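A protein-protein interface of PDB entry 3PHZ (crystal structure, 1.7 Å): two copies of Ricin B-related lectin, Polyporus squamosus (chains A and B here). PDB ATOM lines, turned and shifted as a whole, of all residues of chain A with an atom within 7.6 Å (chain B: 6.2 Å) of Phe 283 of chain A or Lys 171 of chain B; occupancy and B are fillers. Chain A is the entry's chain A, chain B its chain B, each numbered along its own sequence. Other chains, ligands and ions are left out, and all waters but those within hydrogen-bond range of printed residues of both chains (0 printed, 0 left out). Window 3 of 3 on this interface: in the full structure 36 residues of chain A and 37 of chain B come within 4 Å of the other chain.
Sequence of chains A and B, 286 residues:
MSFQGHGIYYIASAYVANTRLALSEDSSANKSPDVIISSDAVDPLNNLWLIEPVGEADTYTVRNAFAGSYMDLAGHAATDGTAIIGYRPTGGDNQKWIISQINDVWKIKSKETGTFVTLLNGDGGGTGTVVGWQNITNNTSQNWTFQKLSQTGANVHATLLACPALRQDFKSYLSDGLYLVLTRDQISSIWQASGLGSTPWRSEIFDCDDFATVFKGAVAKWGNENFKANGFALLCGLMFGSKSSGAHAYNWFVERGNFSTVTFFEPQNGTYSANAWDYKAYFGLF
N of Tyr 173 of chain B is in hydrogen-bond range of O of Phe 286 of chain B (3.0 Å). The backbone carbonyl oxygen of Leu 285 of chain A is in hydrogen-bond range of the backbone NH of Leu 238 of chain A (2.8 Å). The backbone carbonyl oxygen of Gly 241 of chain A is in hydrogen-bond range of the backbone NH of His 248 of chain A (2.8 Å). N of Phe 240 of chain A sits at hydrogen-bond distance from O of Phe 283 of chain A (2.8 Å). N of Phe 286 of chain B is in hydrogen-bond range of O of Lys 171 of chain B (3.1 Å). The backbone carbonyl oxygen of Phe 240 of chain A lies within hydrogen-bond range of the backbone NH of Tyr 282 of chain A (3.0 Å).
The side-chain hydroxyl of Tyr 173 of chain B sits close to the backbone NH of His 248 of chain A, at 3.4 Å.
Of the 10 printed residues of chain B, 4 touch a printed residue of chain A. Printed residues of chain B that touch a printed residue of chain A: Lys 171, Tyr 173, Phe 283 and Leu 285. Hydrophobic or aromatic side chains of chain B within 4 Å of the printed part of chain A: Tyr 173, Phe 283 and Leu 285. Of the 19 printed residues of chain A, 5 touch a printed residue of chain B. Printed residues of chain A that touch a printed residue of chain B: Lys 171, Phe 240, His 248, Phe 283 and Leu 285.
Of chain B, only Lys 171 (3.6 Å), Phe 283 (3.8 Å) and Leu 285 (3.7 Å) come within 4 Å of Phe 283 of chain A. Of chain A, only Phe 283 (3.6 Å) comes within 4 Å of Lys 171 of chain B. Of the printed residues of chain A, Phe 283 of chain B touches Lys 171 (3.2 Å), Phe 283 (3.8 Å) and Leu 285 (3.8 Å). Of the printed residues of chain A, Leu 285 of chain B touches Phe 283. Of the printed residues of chain B, Lys 171 of chain A touches Phe 283. Phe 170 of chain A touches none of the printed residues of chain B. The nearest residue of chain B that does not touch Phe 283 of chain A is Gly 284 of chain B (5.0 Å).
Among the printed residues, merely in contact across the chains: Lys 171 of chain A with Phe 283 of chain B, Phe 283 of chain A with Lys 171 of chain B, Phe 240 of chain A with Tyr 173 of chain B, Phe 283 of chain A with Leu 285 of chain B, Phe 283 of chain A with Phe 283 of chain B and Leu 285 of chain A with Phe 283 of chain B.
Lys 171 of chain A touches Phe 283 of chain B, and with the chains exchanged Phe 283 of chain A touches Lys 171 of chain B. Phe 283 of chain B touches its own counterpart, Phe 283 of chain A. Phe 283 of chain A touches Leu 285 of chain B, and with the chains exchanged Leu 285 of chain A touches Phe 283 of chain B. Positions printed for both chains: 169, 170, 171, 283, 284 and 285.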
ATOM      1  N   LEU A 166       9.306   0.918  -2.532  1.00  0.00           N
ATOM      2  CA  LEU A 166       8.473   2.053  -3.034  1.00  0.00           C
ATOM      3  C   LEU A 166       8.336   2.049  -4.581  1.00  0.00           C
ATOM      4  O   LEU A 166       7.229   2.145  -5.100  1.00  0.00           O
ATOM      5  CB  LEU A 166       9.107   3.402  -2.592  1.00  0.00           C
ATOM      6  CG  LEU A 166       9.041   3.628  -1.074  1.00  0.00           C
ATOM      7  CD1 LEU A 166       9.862   4.933  -0.806  1.00  0.00           C
ATOM      8  CD2 LEU A 166       7.593   3.746  -0.620  1.00  0.00           C
ATOM      9  N   GLN A 168       8.644   4.354  -6.724  1.00  0.00           N
ATOM     10  CA  GLN A 168       7.779   5.464  -7.133  1.00  0.00           C
ATOM     11  C   GLN A 168       8.384   6.730  -6.543  1.00  0.00           C
ATOM     12  O   GLN A 168       9.216   6.671  -5.629  1.00  0.00           O
ATOM     13  CB  GLN A 168       6.363   5.251  -6.584  1.00  0.00           C
ATOM     14  CG  GLN A 168       6.215   5.468  -5.027  1.00  0.00           C
ATOM     15  CD  GLN A 168       4.890   4.911  -4.527  1.00  0.00           C
ATOM     16  OE1 GLN A 168       3.876   5.631  -4.511  1.00  0.00           O
ATOM     17  NE2 GLN A 168       4.862   3.582  -4.189  1.00  0.00           N
ATOM     18  N   ASP A 169       8.018   7.878  -7.104  1.00  0.00           N
ATOM     19  CA  ASP A 169       8.506   9.131  -6.567  1.00  0.00           C
ATOM     20  C   ASP A 169       7.392   9.857  -5.787  1.00  0.00           C
ATOM     21  O   ASP A 169       6.197   9.603  -5.952  1.00  0.00           O
ATOM     22  CB  ASP A 169       9.013   9.977  -7.739  1.00  0.00           C
ATOM     23  CG  ASP A 169       9.967  11.088  -7.315  1.00  0.00           C
ATOM     24  OD1 ASP A 169      10.307  11.249  -6.079  1.00  0.00           O
ATOM     25  OD2 ASP A 169      10.455  11.772  -8.266  1.00  0.00           O
ATOM     26  N   PHE A 170       7.822  10.687  -4.847  1.00  0.00           N
ATOM     27  CA  PHE A 170       6.941  11.549  -4.078  1.00  0.00           C
ATOM     28  C   PHE A 170       7.264  13.005  -4.369  1.00  0.00           C
ATOM     29  O   PHE A 170       8.420  13.357  -4.480  1.00  0.00           O
ATOM     30  CB  PHE A 170       7.157  11.356  -2.577  1.00  0.00           C
ATOM     31  CG  PHE A 170       6.778   9.968  -2.063  1.00  0.00           C
ATOM     32  CD1 PHE A 170       5.647   9.254  -2.614  1.00  0.00           C
ATOM     33  CD2 PHE A 170       7.524   9.400  -1.037  1.00  0.00           C
ATOM     34  CE1 PHE A 170       5.289   7.933  -2.097  1.00  0.00           C
ATOM     35  CE2 PHE A 170       7.193   8.088  -0.501  1.00  0.00           C
ATOM     36  CZ  PHE A 170       6.065   7.377  -1.071  1.00  0.00           C
ATOM     37  N   LYS A 171       6.252  13.870  -4.298  1.00  0.00           N
ATOM     38  CA  LYS A 171       6.453  15.311  -4.453  1.00  0.00           C
ATOM     39  C   LYS A 171       7.268  15.907  -3.279  1.00  0.00           C
ATOM     40  O   LYS A 171       7.104  15.478  -2.145  1.00  0.00           O
ATOM     41  CB  LYS A 171       5.095  16.020  -4.500  1.00  0.00           C
ATOM     42  CG  LYS A 171       4.442  15.878  -5.927  1.00  0.00           C
ATOM     43  CD  LYS A 171       3.147  16.667  -5.947  1.00  0.00           C
ATOM     44  CE  LYS A 171       2.422  16.666  -7.334  1.00  0.00           C
ATOM     45  NZ  LYS A 171       2.217  15.285  -7.905  1.00  0.00           N
ATOM     46  N   LEU A 238       6.536  11.941   4.557  1.00  0.00           N
ATOM     47  CA  LEU A 238       5.290  11.300   4.928  1.00  0.00           C
ATOM     48  C   LEU A 238       4.950  10.318   3.811  1.00  0.00           C
ATOM     49  O   LEU A 238       5.292  10.581   2.658  1.00  0.00           O
ATOM     50  CB  LEU A 238       4.262  12.466   5.018  1.00  0.00           C
ATOM     51  CG  LEU A 238       2.792  12.352   5.065  1.00  0.00           C
ATOM     52  CD1 LEU A 238       2.335  11.419   6.193  1.00  0.00           C
ATOM     53  CD2 LEU A 238       2.532  13.833   5.465  1.00  0.00           C
ATOM     54  N   MET A 239       4.316   9.193   4.140  1.00  0.00           N
ATOM     55  CA  MET A 239       3.779   8.259   3.120  1.00  0.00           C
ATOM     56  C   MET A 239       2.497   7.666   3.646  1.00  0.00           C
ATOM     57  O   MET A 239       2.304   7.544   4.872  1.00  0.00           O
ATOM     58  CB  MET A 239       4.757   7.169   2.748  1.00  0.00           C
ATOM     59  CG  MET A 239       5.134   6.192   3.828  1.00  0.00           C
ATOM     60  SD  MET A 239       5.296   4.390   3.299  1.00  0.00           S
ATOM     61  CE  MET A 239       3.540   4.397   2.942  1.00  0.00           C
ATOM     62  N   PHE A 240       1.576   7.382   2.719  1.00  0.00           N
ATOM     63  CA  PHE A 240       0.327   6.655   3.030  1.00  0.00           C
ATOM     64  C   PHE A 240       0.434   5.336   2.302  1.00  0.00           C
ATOM     65  O   PHE A 240       0.927   5.284   1.163  1.00  0.00           O
ATOM     66  CB  PHE A 240      -0.927   7.346   2.471  1.00  0.00           C
ATOM     67  CG  PHE A 240      -1.231   8.714   3.053  1.00  0.00           C
ATOM     68  CD1 PHE A 240      -0.641   9.173   4.247  1.00  0.00           C
ATOM     69  CD2 PHE A 240      -2.188   9.524   2.416  1.00  0.00           C
ATOM     70  CE1 PHE A 240      -0.959  10.438   4.779  1.00  0.00           C
ATOM     71  CE2 PHE A 240      -2.534  10.808   2.932  1.00  0.00           C
ATOM     72  CZ  PHE A 240      -1.914  11.262   4.113  1.00  0.00           C
ATOM     73  N   GLY A 241       0.058   4.251   2.968  1.00  0.00           N
ATOM     74  CA  GLY A 241       0.248   2.925   2.415  1.00  0.00           C
ATOM     75  C   GLY A 241      -0.941   2.064   2.765  1.00  0.00           C
ATOM     76  O   GLY A 241      -1.760   2.429   3.659  1.00  0.00           O
ATOM     77  N   SER A 242      -1.063   0.943   2.058  1.00  0.00           N
ATOM     78  CA  SER A 242      -2.128   0.018   2.395  1.00  0.00           C
ATOM     79  C   SER A 242      -1.755  -1.427   2.156  1.00  0.00           C
ATOM     80  O   SER A 242      -0.745  -1.765   1.540  1.00  0.00           O
ATOM     81  CB  SER A 242      -3.419   0.351   1.653  1.00  0.00           C
ATOM     82  OG  SER A 242      -3.248   0.004   0.304  1.00  0.00           O
ATOM     83  N   HIS A 248      -2.598   3.107   6.272  1.00  0.00           N
ATOM     84  CA  HIS A 248      -1.681   3.470   7.361  1.00  0.00           C
ATOM     85  C   HIS A 248      -0.851   4.647   6.872  1.00  0.00           C
ATOM     86  O   HIS A 248      -0.737   4.860   5.649  1.00  0.00           O
ATOM     87  CB  HIS A 248      -0.758   2.316   7.746  1.00  0.00           C
ATOM     88  CG  HIS A 248      -0.299   2.368   9.195  1.00  0.00           C
ATOM     89  ND1 HIS A 248      -0.966   1.706  10.216  1.00  0.00           N
ATOM     90  CD2 HIS A 248       0.749   3.013   9.789  1.00  0.00           C
ATOM     91  CE1 HIS A 248      -0.356   1.942  11.371  1.00  0.00           C
ATOM     92  NE2 HIS A 248       0.665   2.758  11.149  1.00  0.00           N
ATOM     93  N   TYR A 250       2.989   6.654   7.611  1.00  0.00           N
ATOM     94  CA  TYR A 250       4.343   6.549   8.179  1.00  0.00           C
ATOM     95  C   TYR A 250       5.144   7.778   7.875  1.00  0.00           C
ATOM     96  O   TYR A 250       4.818   8.560   6.970  1.00  0.00           O
ATOM     97  CB  TYR A 250       5.099   5.363   7.556  1.00  0.00           C
ATOM     98  CG  TYR A 250       4.527   4.028   7.965  1.00  0.00           C
ATOM     99  CD1 TYR A 250       4.690   3.595   9.282  1.00  0.00           C
ATOM    100  CD2 TYR A 250       3.783   3.240   7.074  1.00  0.00           C
ATOM    101  CE1 TYR A 250       4.167   2.350   9.709  1.00  0.00           C
ATOM    102  CE2 TYR A 250       3.257   1.962   7.502  1.00  0.00           C
ATOM    103  CZ  TYR A 250       3.452   1.554   8.817  1.00  0.00           C
ATOM    104  OH  TYR A 250       2.956   0.362   9.341  1.00  0.00           O
ATOM    105  N   TRP A 252       9.209   8.818   6.858  1.00  0.00           N
ATOM    106  CA  TRP A 252      10.337   8.139   6.207  1.00  0.00           C
ATOM    107  C   TRP A 252      11.563   9.029   6.145  1.00  0.00           C
ATOM    108  O   TRP A 252      11.457  10.262   6.172  1.00  0.00           O
ATOM    109  CB  TRP A 252       9.995   7.501   4.819  1.00  0.00           C
ATOM    110  CG  TRP A 252       9.523   8.488   3.792  1.00  0.00           C
ATOM    111  CD1 TRP A 252       8.211   8.844   3.543  1.00  0.00           C
ATOM    112  CD2 TRP A 252      10.345   9.282   2.926  1.00  0.00           C
ATOM    113  NE1 TRP A 252       8.174   9.822   2.562  1.00  0.00           N
ATOM    114  CE2 TRP A 252       9.476  10.098   2.165  1.00  0.00           C
ATOM    115  CE3 TRP A 252      11.750   9.404   2.738  1.00  0.00           C
ATOM    116  CZ2 TRP A 252       9.961  11.054   1.219  1.00  0.00           C
ATOM    117  CZ3 TRP A 252      12.241  10.326   1.759  1.00  0.00           C
ATOM    118  CH2 TRP A 252      11.343  11.139   1.020  1.00  0.00           C
ATOM    119  N   LYS A 280       2.150  -1.119   1.177  1.00  0.00           N
ATOM    120  CA  LYS A 280       2.563  -0.680  -0.134  1.00  0.00           C
ATOM    121  C   LYS A 280       2.137   0.761  -0.240  1.00  0.00           C
ATOM    122  O   LYS A 280       0.944   1.062  -0.139  1.00  0.00           O
ATOM    123  CB  LYS A 280       1.879  -1.496  -1.239  1.00  0.00           C
ATOM    124  CG  LYS A 280       2.340  -1.032  -2.615  1.00  0.00           C
ATOM    125  CD  LYS A 280       1.470  -1.638  -3.704  1.00  0.00           C
ATOM    126  CE  LYS A 280       2.278  -2.539  -4.633  1.00  0.00           C
ATOM    127  NZ  LYS A 280       1.419  -3.679  -5.135  1.00  0.00           N
ATOM    128  N   ALA A 281       3.100   1.649  -0.449  1.00  0.00           N
ATOM    129  CA  ALA A 281       2.790   3.080  -0.539  1.00  0.00           C
ATOM    130  C   ALA A 281       2.044   3.431  -1.796  1.00  0.00           C
ATOM    131  O   ALA A 281       2.322   2.870  -2.897  1.00  0.00           O
ATOM    132  CB  ALA A 281       4.065   3.890  -0.478  1.00  0.00           C
ATOM    133  N   TYR A 282       1.119   4.381  -1.671  1.00  0.00           N
ATOM    134  CA  TYR A 282       0.448   4.928  -2.849  1.00  0.00           C
ATOM    135  C   TYR A 282       0.539   6.446  -2.857  1.00  0.00           C
ATOM    136  O   TYR A 282       0.063   7.077  -3.813  1.00  0.00           O
ATOM    137  CB  TYR A 282      -1.023   4.433  -2.955  1.00  0.00           C
ATOM    138  CG  TYR A 282      -1.822   4.696  -1.690  1.00  0.00           C
ATOM    139  CD1 TYR A 282      -2.422   5.935  -1.435  1.00  0.00           C
ATOM    140  CD2 TYR A 282      -1.928   3.692  -0.707  1.00  0.00           C
ATOM    141  CE1 TYR A 282      -3.153   6.146  -0.232  1.00  0.00           C
ATOM    142  CE2 TYR A 282      -2.632   3.890   0.481  1.00  0.00           C
ATOM    143  CZ  TYR A 282      -3.232   5.129   0.713  1.00  0.00           C
ATOM    144  OH  TYR A 282      -3.913   5.278   1.909  1.00  0.00           O
ATOM    145  N   PHE A 283       1.093   7.065  -1.784  1.00  0.00           N
ATOM    146  CA  PHE A 283       1.119   8.536  -1.728  1.00  0.00           C
ATOM    147  C   PHE A 283       2.206   8.963  -0.783  1.00  0.00           C
ATOM    148  O   PHE A 283       2.453   8.248   0.175  1.00  0.00           O
ATOM    149  CB  PHE A 283      -0.195   9.061  -1.174  1.00  0.00           C
ATOM    150  CG  PHE A 283      -0.181  10.523  -0.935  1.00  0.00           C
ATOM    151  CD1 PHE A 283      -0.287  11.411  -1.998  1.00  0.00           C
ATOM    152  CD2 PHE A 283       0.013  11.032   0.367  1.00  0.00           C
ATOM    153  CE1 PHE A 283      -0.267  12.797  -1.773  1.00  0.00           C
ATOM    154  CE2 PHE A 283       0.068  12.406   0.598  1.00  0.00           C
ATOM    155  CZ  PHE A 283      -0.092  13.293  -0.475  1.00  0.00           C
ATOM    156  N   GLY A 284       2.833  10.106  -1.023  1.00  0.00           N
ATOM    157  CA  GLY A 284       3.819  10.600   0.002  1.00  0.00           C
ATOM    158  C   GLY A 284       4.322  11.982  -0.351  1.00  0.00           C
ATOM    159  O   GLY A 284       3.958  12.506  -1.365  1.00  0.00           O
ATOM    160  N   LEU A 285       5.173  12.552   0.504  1.00  0.00           N
ATOM    161  CA  LEU A 285       5.566  13.944   0.365  1.00  0.00           C
ATOM    162  C   LEU A 285       6.835  14.133   1.174  1.00  0.00           C
ATOM    163  O   LEU A 285       7.030  13.399   2.160  1.00  0.00           O
ATOM    164  CB  LEU A 285       4.443  14.781   0.984  1.00  0.00           C
ATOM    165  CG  LEU A 285       4.538  16.244   1.257  1.00  0.00           C
ATOM    166  CD1 LEU A 285       4.885  16.950  -0.071  1.00  0.00           C
ATOM    167  CD2 LEU A 285       3.129  16.665   1.759  1.00  0.00           C
ATOM    168  N   HIS B 157     -14.328  16.553  -1.308  1.00  0.00           N
ATOM    169  CA  HIS B 157     -13.689  16.270  -2.638  1.00  0.00           C
ATOM    170  C   HIS B 157     -14.537  16.974  -3.721  1.00  0.00           C
ATOM    171  O   HIS B 157     -13.983  17.591  -4.611  1.00  0.00           O
ATOM    172  CB  HIS B 157     -13.686  14.766  -2.874  1.00  0.00           C
ATOM    173  CG  HIS B 157     -12.630  14.036  -2.084  1.00  0.00           C
ATOM    174  ND1 HIS B 157     -11.294  14.265  -2.292  1.00  0.00           N
ATOM    175  CD2 HIS B 157     -12.709  13.022  -1.179  1.00  0.00           C
ATOM    176  CE1 HIS B 157     -10.577  13.447  -1.531  1.00  0.00           C
ATOM    177  NE2 HIS B 157     -11.406  12.709  -0.819  1.00  0.00           N
ATOM    178  N   ASP B 169      -8.975  18.033  -7.557  1.00  0.00           N
ATOM    179  CA  ASP B 169      -9.201  17.323  -6.294  1.00  0.00           C
ATOM    180  C   ASP B 169      -7.865  17.094  -5.589  1.00  0.00           C
ATOM    181  O   ASP B 169      -6.800  17.069  -6.216  1.00  0.00           O
ATOM    182  CB  ASP B 169      -9.921  16.002  -6.627  1.00  0.00           C
ATOM    183  CG  ASP B 169     -10.678  15.386  -5.421  1.00  0.00           C
ATOM    184  OD1 ASP B 169     -10.632  16.025  -4.336  1.00  0.00           O
ATOM    185  OD2 ASP B 169     -11.289  14.273  -5.559  1.00  0.00           O
ATOM    186  N   PHE B 170      -7.907  16.973  -4.251  1.00  0.00           N
ATOM    187  CA  PHE B 170      -6.756  16.606  -3.466  1.00  0.00           C
ATOM    188  C   PHE B 170      -7.022  15.280  -2.795  1.00  0.00           C
ATOM    189  O   PHE B 170      -8.174  14.979  -2.474  1.00  0.00           O
ATOM    190  CB  PHE B 170      -6.565  17.633  -2.347  1.00  0.00           C
ATOM    191  CG  PHE B 170      -6.163  19.014  -2.863  1.00  0.00           C
ATOM    192  CD1 PHE B 170      -5.288  19.149  -3.964  1.00  0.00           C
ATOM    193  CD2 PHE B 170      -6.601  20.140  -2.175  1.00  0.00           C
ATOM    194  CE1 PHE B 170      -4.922  20.474  -4.428  1.00  0.00           C
ATOM    195  CE2 PHE B 170      -6.248  21.445  -2.573  1.00  0.00           C
ATOM    196  CZ  PHE B 170      -5.396  21.621  -3.719  1.00  0.00           C
ATOM    197  N   LYS B 171      -5.985  14.491  -2.525  1.00  0.00           N
ATOM    198  CA  LYS B 171      -6.153  13.221  -1.829  1.00  0.00           C
ATOM    199  C   LYS B 171      -6.548  13.438  -0.370  1.00  0.00           C
ATOM    200  O   LYS B 171      -6.071  14.390   0.258  1.00  0.00           O
ATOM    201  CB  LYS B 171      -4.820  12.501  -1.824  1.00  0.00           C
ATOM    202  CG  LYS B 171      -4.572  11.767  -3.203  1.00  0.00           C
ATOM    203  CD  LYS B 171      -3.655  10.548  -3.065  1.00  0.00           C
ATOM    204  CE  LYS B 171      -3.052  10.154  -4.449  1.00  0.00           C
ATOM    205  NZ  LYS B 171      -2.947  11.265  -5.426  1.00  0.00           N
ATOM    206  N   SER B 172      -7.368  12.545   0.172  1.00  0.00           N
ATOM    207  CA  SER B 172      -7.631  12.593   1.627  1.00  0.00           C
ATOM    208  C   SER B 172      -7.061  11.318   2.222  1.00  0.00           C
ATOM    209  O   SER B 172      -7.045  10.253   1.607  1.00  0.00           O
ATOM    210  CB  SER B 172      -9.135  12.666   1.922  1.00  0.00           C
ATOM    211  OG  SER B 172      -9.816  11.610   1.222  1.00  0.00           O
ATOM    212  N   TYR B 173      -6.519  11.429   3.413  1.00  0.00           N
ATOM    213  CA  TYR B 173      -6.087  10.212   4.094  1.00  0.00           C
ATOM    214  C   TYR B 173      -7.216   9.237   4.353  1.00  0.00           C
ATOM    215  O   TYR B 173      -7.087   7.993   4.094  1.00  0.00           O
ATOM    216  CB  TYR B 173      -5.396  10.593   5.435  1.00  0.00           C
ATOM    217  CG  TYR B 173      -5.041   9.295   6.150  1.00  0.00           C
ATOM    218  CD1 TYR B 173      -4.007   8.496   5.663  1.00  0.00           C
ATOM    219  CD2 TYR B 173      -5.752   8.853   7.279  1.00  0.00           C
ATOM    220  CE1 TYR B 173      -3.665   7.261   6.268  1.00  0.00           C
ATOM    221  CE2 TYR B 173      -5.406   7.617   7.890  1.00  0.00           C
ATOM    222  CZ  TYR B 173      -4.383   6.840   7.379  1.00  0.00           C
ATOM    223  OH  TYR B 173      -4.044   5.605   7.975  1.00  0.00           O
ATOM    224  N   PHE B 283      -0.930  21.117  -5.799  1.00  0.00           N
ATOM    225  CA  PHE B 283      -0.811  19.944  -4.952  1.00  0.00           C
ATOM    226  C   PHE B 283      -1.534  20.196  -3.642  1.00  0.00           C
ATOM    227  O   PHE B 283      -1.587  21.339  -3.213  1.00  0.00           O
ATOM    228  CB  PHE B 283       0.671  19.643  -4.668  1.00  0.00           C
ATOM    229  CG  PHE B 283       0.863  18.597  -3.558  1.00  0.00           C
ATOM    230  CD1 PHE B 283       0.869  17.250  -3.848  1.00  0.00           C
ATOM    231  CD2 PHE B 283       0.951  19.005  -2.207  1.00  0.00           C
ATOM    232  CE1 PHE B 283       1.038  16.278  -2.804  1.00  0.00           C
ATOM    233  CE2 PHE B 283       1.061  18.065  -1.161  1.00  0.00           C
ATOM    234  CZ  PHE B 283       1.135  16.694  -1.473  1.00  0.00           C
ATOM    235  N   GLY B 284      -2.034  19.139  -2.997  1.00  0.00           N
ATOM    236  CA  GLY B 284      -2.823  19.385  -1.727  1.00  0.00           C
ATOM    237  C   GLY B 284      -3.230  18.076  -1.083  1.00  0.00           C
ATOM    238  O   GLY B 284      -3.158  16.995  -1.695  1.00  0.00           O
ATOM    239  N   LEU B 285      -3.672  18.161   0.177  1.00  0.00           N
ATOM    240  CA  LEU B 285      -4.136  16.952   0.845  1.00  0.00           C
ATOM    241  C   LEU B 285      -5.044  17.374   2.012  1.00  0.00           C
ATOM    242  O   LEU B 285      -4.984  18.518   2.439  1.00  0.00           O
ATOM    243  CB  LEU B 285      -2.986  16.046   1.338  1.00  0.00           C
ATOM    244  CG  LEU B 285      -2.025  16.515   2.377  1.00  0.00           C
ATOM    245  CD1 LEU B 285      -2.731  16.695   3.682  1.00  0.00           C
ATOM    246  CD2 LEU B 285      -0.985  15.349   2.621  1.00  0.00           C
ATOM    247  N   PHE B 286      -5.827  16.431   2.513  1.00  0.00           N
ATOM    248  CA  PHE B 286      -6.608  16.635   3.758  1.00  0.00           C
ATOM    249  C   PHE B 286      -6.840  15.312   4.424  1.00  0.00           C
ATOM    250  O   PHE B 286      -6.246  14.327   3.983  1.00  0.00           O
ATOM    251  CB  PHE B 286      -7.920  17.404   3.551  1.00  0.00           C
ATOM    252  CG  PHE B 286      -8.970  16.695   2.732  1.00  0.00           C
ATOM    253  CD1 PHE B 286     -10.123  16.210   3.328  1.00  0.00           C
ATOM    254  CD2 PHE B 286      -8.838  16.642   1.331  1.00  0.00           C
ATOM    255  CE1 PHE B 286     -11.169  15.659   2.601  1.00  0.00           C
ATOM    256  CE2 PHE B 286      -9.851  16.094   0.573  1.00  0.00           C
ATOM    257  CZ  PHE B 286     -11.044  15.636   1.162  1.00  0.00           C
ATOM    258  OXT PHE B 286      -7.560  15.208   5.400  1.00  0.00           O
